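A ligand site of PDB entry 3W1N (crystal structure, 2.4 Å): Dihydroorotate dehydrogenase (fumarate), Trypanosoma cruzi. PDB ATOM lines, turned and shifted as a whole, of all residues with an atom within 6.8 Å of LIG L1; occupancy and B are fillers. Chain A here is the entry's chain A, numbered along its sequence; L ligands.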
ATOM      1  N   ALA A  20      32.645 -19.440 -31.470  1.00  0.00           N
ATOM      2  CA  ALA A  20      31.714 -18.427 -30.992  1.00  0.00           C
ATOM      3  C   ALA A  20      31.965 -18.157 -29.536  1.00  0.00           C
ATOM      4  O   ALA A  20      32.194 -19.070 -28.729  1.00  0.00           O
ATOM      5  CB  ALA A  20      30.278 -18.866 -31.224  1.00  0.00           C
ATOM      6  N   GLY A  21      31.957 -16.892 -29.186  1.00  0.00           N
ATOM      7  CA  GLY A  21      32.103 -16.496 -27.763  1.00  0.00           C
ATOM      8  C   GLY A  21      33.469 -15.903 -27.460  1.00  0.00           C
ATOM      9  O   GLY A  21      33.596 -15.102 -26.524  1.00  0.00           O
ATOM     10  N   LYS A  44      29.511 -13.299 -31.242  1.00  0.00           N
ATOM     11  CA  LYS A  44      29.092 -13.828 -29.941  1.00  0.00           C
ATOM     12  C   LYS A  44      27.634 -14.270 -30.048  1.00  0.00           C
ATOM     13  O   LYS A  44      26.822 -13.579 -30.699  1.00  0.00           O
ATOM     14  CB  LYS A  44      29.294 -12.774 -28.834  1.00  0.00           C
ATOM     15  CG  LYS A  44      28.645 -13.120 -27.467  1.00  0.00           C
ATOM     16  CD  LYS A  44      29.300 -14.305 -26.774  1.00  0.00           C
ATOM     17  CE  LYS A  44      28.450 -14.864 -25.629  1.00  0.00           C
ATOM     18  NZ  LYS A  44      29.152 -15.960 -24.874  1.00  0.00           N
ATOM     19  N   SER A  45      27.294 -15.409 -29.456  1.00  0.00           N
ATOM     20  CA  SER A  45      25.896 -15.857 -29.405  1.00  0.00           C
ATOM     21  C   SER A  45      25.050 -14.798 -28.742  1.00  0.00           C
ATOM     22  O   SER A  45      25.393 -14.361 -27.659  1.00  0.00           O
ATOM     23  CB  SER A  45      25.711 -17.117 -28.565  1.00  0.00           C
ATOM     24  OG  SER A  45      26.219 -18.245 -29.196  1.00  0.00           O
ATOM     25  N   CYS A  46      23.907 -14.463 -29.340  1.00  0.00           N
ATOM     26  CA  CYS A  46      23.105 -13.332 -28.863  1.00  0.00           C
ATOM     27  C   CYS A  46      21.670 -13.642 -28.503  1.00  0.00           C
ATOM     28  O   CYS A  46      21.096 -14.653 -28.896  1.00  0.00           O
ATOM     29  CB  CYS A  46      23.128 -12.171 -29.845  1.00  0.00           C
ATOM     30  SG  CYS A  46      22.374 -12.470 -31.449  1.00  0.00           S
ATOM     31  N   ASN A  54      26.813 -13.652 -16.250  1.00  0.00           N
ATOM     32  CA  ASN A  54      26.986 -14.057 -14.863  1.00  0.00           C
ATOM     33  C   ASN A  54      28.037 -13.196 -14.193  1.00  0.00           C
ATOM     34  O   ASN A  54      28.786 -12.499 -14.882  1.00  0.00           O
ATOM     35  CB  ASN A  54      27.368 -15.537 -14.781  1.00  0.00           C
ATOM     36  CG  ASN A  54      26.249 -16.458 -15.252  1.00  0.00           C
ATOM     37  OD1 ASN A  54      25.063 -16.087 -15.238  1.00  0.00           O
ATOM     38  ND2 ASN A  54      26.610 -17.654 -15.687  1.00  0.00           N
ATOM     39  N   ASN A  68      34.277 -22.201 -18.192  1.00  0.00           N
ATOM     40  CA  ASN A  68      33.494 -20.955 -18.182  1.00  0.00           C
ATOM     41  C   ASN A  68      32.033 -21.100 -17.914  1.00  0.00           C
ATOM     42  O   ASN A  68      31.432 -22.074 -18.212  1.00  0.00           O
ATOM     43  CB  ASN A  68      33.666 -20.168 -19.496  1.00  0.00           C
ATOM     44  CG  ASN A  68      32.676 -20.594 -20.589  1.00  0.00           C
ATOM     45  OD1 ASN A  68      31.520 -20.142 -20.632  1.00  0.00           O
ATOM     46  ND2 ASN A  68      33.132 -21.455 -21.480  1.00  0.00           N
ATOM     47  N   SER A  69      31.488 -20.086 -17.291  1.00  0.00           N
ATOM     48  CA  SER A  69      30.065 -19.908 -17.157  1.00  0.00           C
ATOM     49  C   SER A  69      29.810 -18.436 -17.387  1.00  0.00           C
ATOM     50  O   SER A  69      29.404 -17.719 -16.481  1.00  0.00           O
ATOM     51  CB  SER A  69      29.591 -20.354 -15.788  1.00  0.00           C
ATOM     52  OG  SER A  69      28.176 -20.116 -15.665  1.00  0.00           O
ATOM     53  N   MET A  70      30.110 -18.002 -18.617  1.00  0.00           N
ATOM     54  CA  MET A  70      29.984 -16.585 -19.009  1.00  0.00           C
ATOM     55  C   MET A  70      28.534 -16.121 -18.780  1.00  0.00           C
ATOM     56  O   MET A  70      28.264 -15.009 -18.255  1.00  0.00           O
ATOM     57  CB  MET A  70      30.332 -16.373 -20.481  1.00  0.00           C
ATOM     58  CG  MET A  70      31.727 -16.766 -20.931  1.00  0.00           C
ATOM     59  SD  MET A  70      33.068 -16.194 -19.865  1.00  0.00           S
ATOM     60  CE  MET A  70      33.074 -14.456 -20.285  1.00  0.00           C
ATOM     61  N   GLY A  71      27.623 -17.001 -19.159  1.00  0.00           N
ATOM     62  CA  GLY A  71      26.203 -16.796 -19.006  1.00  0.00           C
ATOM     63  C   GLY A  71      25.615 -15.912 -20.083  1.00  0.00           C
ATOM     64  O   GLY A  71      24.686 -15.165 -19.811  1.00  0.00           O
ATOM     65  N   LEU A  72      26.187 -15.967 -21.270  1.00  0.00           N
ATOM     66  CA  LEU A  72      25.563 -15.400 -22.455  1.00  0.00           C
ATOM     67  C   LEU A  72      25.577 -13.876 -22.387  1.00  0.00           C
ATOM     68  O   LEU A  72      24.638 -13.219 -22.799  1.00  0.00           O
ATOM     69  CB  LEU A  72      24.140 -16.000 -22.582  1.00  0.00           C
ATOM     70  CG  LEU A  72      23.400 -16.092 -23.916  1.00  0.00           C
ATOM     71  CD1 LEU A  72      24.379 -15.989 -25.094  1.00  0.00           C
ATOM     72  CD2 LEU A  72      22.545 -17.375 -23.985  1.00  0.00           C
ATOM     73  N   PRO A  73      26.667 -13.283 -21.858  1.00  0.00           N
ATOM     74  CA  PRO A  73      26.674 -11.811 -22.029  1.00  0.00           C
ATOM     75  C   PRO A  73      26.827 -11.412 -23.485  1.00  0.00           C
ATOM     76  O   PRO A  73      27.658 -11.948 -24.174  1.00  0.00           O
ATOM     77  CB  PRO A  73      27.957 -11.341 -21.316  1.00  0.00           C
ATOM     78  CG  PRO A  73      28.790 -12.543 -21.194  1.00  0.00           C
ATOM     79  CD  PRO A  73      27.982 -13.808 -21.477  1.00  0.00           C
ATOM     80  N   SER A 100      21.467 -17.377 -29.664  1.00  0.00           N
ATOM     81  CA  SER A 100      21.184 -18.323 -28.574  1.00  0.00           C
ATOM     82  C   SER A 100      19.999 -17.885 -27.715  1.00  0.00           C
ATOM     83  O   SER A 100      20.105 -17.796 -26.501  1.00  0.00           O
ATOM     84  CB  SER A 100      22.424 -18.548 -27.715  1.00  0.00           C
ATOM     85  OG  SER A 100      22.207 -19.660 -26.858  1.00  0.00           O
ATOM     86  N   ASN A 128      22.644 -21.817 -31.981  1.00  0.00           N
ATOM     87  CA  ASN A 128      23.266 -22.410 -30.816  1.00  0.00           C
ATOM     88  C   ASN A 128      22.290 -23.262 -29.984  1.00  0.00           C
ATOM     89  O   ASN A 128      21.449 -22.735 -29.277  1.00  0.00           O
ATOM     90  CB  ASN A 128      23.870 -21.317 -29.929  1.00  0.00           C
ATOM     91  CG  ASN A 128      24.703 -21.885 -28.783  1.00  0.00           C
ATOM     92  OD1 ASN A 128      24.766 -23.113 -28.581  1.00  0.00           O
ATOM     93  ND2 ASN A 128      25.364 -20.998 -28.049  1.00  0.00           N
ATOM     94  N   SER A 130      23.254 -25.418 -27.562  1.00  0.00           N
ATOM     95  CA  SER A 130      24.080 -26.080 -26.563  1.00  0.00           C
ATOM     96  C   SER A 130      24.733 -25.211 -25.487  1.00  0.00           C
ATOM     97  O   SER A 130      25.706 -25.649 -24.927  1.00  0.00           O
ATOM     98  CB  SER A 130      25.154 -26.876 -27.302  1.00  0.00           C
ATOM     99  OG  SER A 130      25.710 -26.122 -28.367  1.00  0.00           O
ATOM    100  N   CYS A 131      24.222 -24.015 -25.193  1.00  0.00           N
ATOM    101  CA  CYS A 131      24.734 -23.264 -23.991  1.00  0.00           C
ATOM    102  C   CYS A 131      24.491 -24.122 -22.744  1.00  0.00           C
ATOM    103  O   CYS A 131      23.329 -24.369 -22.377  1.00  0.00           O
ATOM    104  CB  CYS A 131      24.062 -21.887 -23.808  1.00  0.00           C
ATOM    105  SG  CYS A 131      24.666 -20.882 -22.392  1.00  0.00           S
ATOM    106  N   PRO A 132      25.580 -24.617 -22.094  1.00  0.00           N
ATOM    107  CA  PRO A 132      25.451 -25.383 -20.846  1.00  0.00           C
ATOM    108  C   PRO A 132      25.338 -24.509 -19.585  1.00  0.00           C
ATOM    109  O   PRO A 132      25.220 -25.078 -18.470  1.00  0.00           O
ATOM    110  CB  PRO A 132      26.768 -26.163 -20.804  1.00  0.00           C
ATOM    111  CG  PRO A 132      27.758 -25.169 -21.335  1.00  0.00           C
ATOM    112  CD  PRO A 132      27.022 -24.402 -22.423  1.00  0.00           C
ATOM    113  N   ASN A 133      25.350 -23.171 -19.737  1.00  0.00           N
ATOM    114  CA  ASN A 133      25.656 -22.228 -18.612  1.00  0.00           C
ATOM    115  C   ASN A 133      24.562 -21.318 -18.036  1.00  0.00           C
ATOM    116  O   ASN A 133      24.813 -20.582 -17.077  1.00  0.00           O
ATOM    117  CB  ASN A 133      26.866 -21.367 -19.004  1.00  0.00           C
ATOM    118  CG  ASN A 133      28.152 -22.167 -19.022  1.00  0.00           C
ATOM    119  OD1 ASN A 133      28.365 -23.025 -18.166  1.00  0.00           O
ATOM    120  ND2 ASN A 133      29.022 -21.877 -19.992  1.00  0.00           N
ATOM    121  N   VAL A 134      23.366 -21.326 -18.614  1.00  0.00           N
ATOM    122  CA  VAL A 134      22.299 -20.470 -18.087  1.00  0.00           C
ATOM    123  C   VAL A 134      21.464 -21.324 -17.115  1.00  0.00           C
ATOM    124  O   VAL A 134      20.969 -22.370 -17.508  1.00  0.00           O
ATOM    125  CB  VAL A 134      21.467 -19.820 -19.217  1.00  0.00           C
ATOM    126  CG1 VAL A 134      20.280 -19.053 -18.637  1.00  0.00           C
ATOM    127  CG2 VAL A 134      22.325 -18.853 -20.023  1.00  0.00           C
ATOM    128  N   LYS A 165      25.160 -25.415 -33.690  1.00  0.00           N
ATOM    129  CA  LYS A 165      26.248 -25.635 -32.759  1.00  0.00           C
ATOM    130  C   LYS A 165      25.808 -26.688 -31.719  1.00  0.00           C
ATOM    131  O   LYS A 165      24.912 -26.403 -30.873  1.00  0.00           O
ATOM    132  CB  LYS A 165      26.586 -24.318 -32.057  1.00  0.00           C
ATOM    133  CG  LYS A 165      27.753 -24.432 -31.099  1.00  0.00           C
ATOM    134  CD  LYS A 165      29.080 -24.416 -31.856  1.00  0.00           C
ATOM    135  CE  LYS A 165      30.259 -24.437 -30.908  1.00  0.00           C
ATOM    136  NZ  LYS A 165      30.528 -23.098 -30.390  1.00  0.00           N
ATOM    137  N   ASN A 195      30.402 -27.712 -28.733  1.00  0.00           N
ATOM    138  CA  ASN A 195      30.381 -26.692 -27.684  1.00  0.00           C
ATOM    139  C   ASN A 195      31.206 -27.223 -26.526  1.00  0.00           C
ATOM    140  O   ASN A 195      31.805 -28.295 -26.608  1.00  0.00           O
ATOM    141  CB  ASN A 195      28.931 -26.377 -27.231  1.00  0.00           C
ATOM    142  CG  ASN A 195      28.749 -24.918 -26.778  1.00  0.00           C
ATOM    143  OD1 ASN A 195      29.428 -24.442 -25.865  1.00  0.00           O
ATOM    144  ND2 ASN A 195      27.791 -24.232 -27.391  1.00  0.00           N
ATOM    145  N   SER A 196      31.248 -26.486 -25.423  1.00  0.00           N
ATOM    146  CA  SER A 196      32.126 -26.894 -24.338  1.00  0.00           C
ATOM    147  C   SER A 196      31.516 -28.099 -23.679  1.00  0.00           C
ATOM    148  O   SER A 196      30.302 -28.338 -23.765  1.00  0.00           O
ATOM    149  CB  SER A 196      32.403 -25.745 -23.366  1.00  0.00           C
ATOM    150  OG  SER A 196      31.223 -25.184 -22.845  1.00  0.00           O
ATOM    151  N   VAL A 197      32.377 -28.900 -23.085  1.00  0.00           N
ATOM    152  CA  VAL A 197      31.935 -30.059 -22.344  1.00  0.00           C
ATOM    153  C   VAL A 197      31.369 -29.550 -21.025  1.00  0.00           C
ATOM    154  O   VAL A 197      32.054 -28.906 -20.224  1.00  0.00           O
ATOM    155  CB  VAL A 197      33.102 -31.024 -22.145  1.00  0.00           C
ATOM    156  CG1 VAL A 197      32.701 -32.222 -21.322  1.00  0.00           C
ATOM    157  CG2 VAL A 197      33.618 -31.476 -23.509  1.00  0.00           C
ATOM    158  N   GLY A 219      31.054 -25.098 -14.719  1.00  0.00           N
ATOM    159  CA  GLY A 219      31.079 -24.438 -16.048  1.00  0.00           C
ATOM    160  C   GLY A 219      31.522 -25.371 -17.184  1.00  0.00           C
ATOM    161  O   GLY A 219      31.955 -26.520 -16.958  1.00  0.00           O
ATOM    162  N   GLY A 220      31.406 -24.865 -18.410  1.00  0.00           N
ATOM    163  CA  GLY A 220      31.869 -25.589 -19.581  1.00  0.00           C
ATOM    164  C   GLY A 220      33.394 -25.640 -19.765  1.00  0.00           C
ATOM    165  O   GLY A 220      34.107 -24.605 -19.603  1.00  0.00           O
ATOM    166  N   LEU A 221      33.889 -26.823 -20.140  1.00  0.00           N
ATOM    167  CA  LEU A 221      35.318 -27.039 -20.350  1.00  0.00           C
ATOM    168  C   LEU A 221      35.689 -26.939 -21.827  1.00  0.00           C
ATOM    169  O   LEU A 221      34.986 -27.471 -22.685  1.00  0.00           O
ATOM    170  CB  LEU A 221      35.717 -28.398 -19.836  1.00  0.00           C
ATOM    171  CG  LEU A 221      35.297 -28.820 -18.436  1.00  0.00           C
ATOM    172  CD1 LEU A 221      35.544 -30.297 -18.230  1.00  0.00           C
ATOM    173  CD2 LEU A 221      36.037 -28.007 -17.388  1.00  0.00           C
HETATM  174  O1  LIG L   1      28.115 -18.719 -21.285  1.00  0.00           O
HETATM  175  C1  LIG L   1      28.408 -18.567 -22.483  1.00  0.00           C
HETATM  176  O2  LIG L   1      28.181 -17.457 -22.970  1.00  0.00           O
HETATM  177  C2  LIG L   1      28.715 -19.722 -23.212  1.00  0.00           C
HETATM  178  C3  LIG L   1      27.885 -20.147 -24.259  1.00  0.00           C
HETATM  179  I1  LIG L   1      26.233 -18.932 -24.879  1.00  0.00           I
HETATM  180  C4  LIG L   1      28.102 -21.349 -24.910  1.00  0.00           C
HETATM  181  O3  LIG L   1      27.369 -21.707 -25.827  1.00  0.00           O
HETATM  182  N1  LIG L   1      29.172 -22.134 -24.506  1.00  0.00           N
HETATM  183  C5  LIG L   1      29.981 -21.704 -23.458  1.00  0.00           C
HETATM  184  O4  LIG L   1      30.900 -22.430 -23.111  1.00  0.00           O
HETATM  185  N2  LIG L   1      29.763 -20.502 -22.807  1.00  0.00           N
HETATM  186  N1  LG2 L   2      29.960 -21.222 -27.780  1.00  0.00           N
HETATM  187  C1  LG2 L   2      28.852 -20.724 -28.355  1.00  0.00           C
HETATM  188  O1  LG2 L   2      28.171 -21.432 -29.156  1.00  0.00           O
HETATM  189  N2  LG2 L   2      28.413 -19.502 -28.124  1.00  0.00           N
HETATM  190  C2  LG2 L   2      29.035 -18.661 -27.311  1.00  0.00           C
HETATM  191  O2  LG2 L   2      28.592 -17.497 -27.131  1.00  0.00           O
HETATM  192  C3  LG2 L   2      30.240 -19.143 -26.613  1.00  0.00           C
HETATM  193  N3  LG2 L   2      30.916 -18.375 -25.771  1.00  0.00           N
HETATM  194  C4  LG2 L   2      32.090 -18.834 -25.234  1.00  0.00           C
HETATM  195  C5  LG2 L   2      32.828 -18.020 -24.386  1.00  0.00           C
HETATM  196  C6  LG2 L   2      33.995 -18.461 -23.812  1.00  0.00           C
HETATM  197  C7  LG2 L   2      34.722 -17.538 -22.875  1.00  0.00           C
HETATM  198  C8  LG2 L   2      34.464 -19.858 -24.080  1.00  0.00           C
HETATM  199  C9  LG2 L   2      35.732 -20.406 -23.465  1.00  0.00           C
HETATM  200  C10 LG2 L   2      33.738 -20.682 -24.921  1.00  0.00           C
HETATM  201  C11 LG2 L   2      32.589 -20.219 -25.519  1.00  0.00           C
HETATM  202  N4  LG2 L   2      31.832 -21.043 -26.349  1.00  0.00           N
HETATM  203  C12 LG2 L   2      30.667 -20.518 -26.917  1.00  0.00           C
HETATM  204  C13 LG2 L   2      32.264 -22.384 -26.684  1.00  0.00           C
HETATM  205  C14 LG2 L   2      33.294 -22.321 -27.769  1.00  0.00           C
HETATM  206  O3  LG2 L   2      32.648 -21.723 -28.901  1.00  0.00           O
HETATM  207  C15 LG2 L   2      33.809 -23.697 -28.134  1.00  0.00           C
HETATM  208  O4  LG2 L   2      32.682 -24.410 -28.651  1.00  0.00           O
HETATM  209  C16 LG2 L   2      34.468 -24.421 -26.970  1.00  0.00           C
HETATM  210  O5  LG2 L   2      35.153 -23.495 -26.138  1.00  0.00           O
HETATM  211  C17 LG2 L   2      35.462 -25.555 -27.296  1.00  0.00           C
HETATM  212  O6  LG2 L   2      36.533 -25.145 -28.159  1.00  0.00           O
HETATM  213  P1  LG2 L   2      37.973 -24.875 -27.477  1.00  0.00           P
HETATM  214  O7  LG2 L   2      38.819 -24.272 -28.565  1.00  0.00           O
HETATM  215  O8  LG2 L   2      38.380 -26.253 -27.002  1.00  0.00           O
HETATM  216  O9  LG2 L   2      37.699 -23.910 -26.348  1.00  0.00           O
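N of Ser 45 lies close to O2 of LG2 L2.
The side-chain hydroxyl (OG) of Ser 196 is in hydrogen-bond range of an oxygen (O4) of LIG L1, 2.8 Å away.
The side-chain amide nitrogen (ND2) of Asn 128 lies within hydrogen-bond range of an oxygen (O1) of LG2 L2.
O2 of LIG L1 lies within salt-bridge range of NZ of Lys 44 (2.6 Å).
The side-chain amide oxygen (OD1) of Asn 68 is in hydrogen-bond range of a nitrogen (N2) of LIG L1, at 2.8 Å.
The side-chain amino group (NZ) of Lys 44 lies within hydrogen-bond range of an oxygen (O2) of LG2 L2.
An oxygen (O3) of LIG L1 sits at hydrogen-bond distance from the side-chain amide nitrogen (ND2) of Asn 128, at 3.1 Å.
The backbone NH (N) of Gly 71 is in hydrogen-bond range of an oxygen (O1) of LIG L1 (2.8 Å).
The backbone carbonyl oxygen (O) of Ala 20 sits at hydrogen-bond distance from an oxygen (O3) of LG2 L2 (2.7 Å).
The backbone NH of Leu 72 lies within hydrogen-bond range of an oxygen (O2) of LIG L1 (3.0 Å).
The side-chain amino group (NZ) of Lys 165 lies within hydrogen-bond range of an oxygen (O3) of LG2 L2 (2.9 Å).
OD1 of Asn 195 sits at hydrogen-bond distance from N1 of LIG L1 (2.7 Å).
An oxygen (O1) of LIG L1 sits close to the backbone NH (N) of Met 70 (3.4 Å).
O3 of LG2 L2 is in hydrogen-bond range of N of Ala 20.
The side-chain hydroxyl (OG) of Ser 45 is in hydrogen-bond range of a nitrogen (N2) of LG2 L2 (2.7 Å).
The side-chain amide nitrogen of Asn 133 sits close to a nitrogen (N2) of LIG L1 (3.2 Å).
An oxygen (O1) of LG2 L2 is in hydrogen-bond range of the side-chain amide nitrogen of Asn 195 (3.3 Å).
N2 of LG2 L2 sits close to O3 of LIG L1 (3.4 Å).
O of Asn 68 is in hydrogen-bond range of ND2 of Asn 133 (3.0 Å).
The backbone NH (N) of Asn 54 is in hydrogen-bond range of the backbone carbonyl oxygen (O) of Met 70.
N of Ser 130 lies within hydrogen-bond range of OD1 of Asn 128 (2.9 Å).
The side-chain amide nitrogen (ND2) of Asn 195 is in hydrogen-bond range of the side-chain amide oxygen (OD1) of Asn 128 (3.4 Å).
The side-chain hydroxyl (OG) of Ser 45 sits at hydrogen-bond distance from the side-chain amide nitrogen (ND2) of Asn 128.
N of Asn 133 sits close to SG of Cys 131 (3.6 Å).
The backbone carbonyl oxygen (O) of Gly 220 sits at hydrogen-bond distance from the backbone NH (N) of Asn 68 (2.8 Å).
The side-chain amide nitrogen (ND2) of Asn 195 is in hydrogen-bond range of the side-chain hydroxyl (OG) of Ser 130 (3.0 Å).
Residues that only touch LIG L1: Cys 131 (3.5 Å), Pro 132 (3.8 Å) and Pro 73 (3.9 Å).
Hydrophobic or aromatic side chains that line LIG L1: Met 70, Leu 72, Pro 73 and Pro 132.
12 residues have an atom within 4 Å of LIG L1: Lys 44, Asn 68, Met 70, Gly 71, Leu 72, Pro 73, Asn 128, Cys 131, Pro 132, Asn 133, Asn 195 and Ser 196.
Along chain A the residues within 4 Å of LIG L1 span positions 44 to 196.
The nearest printed residue that does not touch LIG L1 is Ser 45 (4.1 Å).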
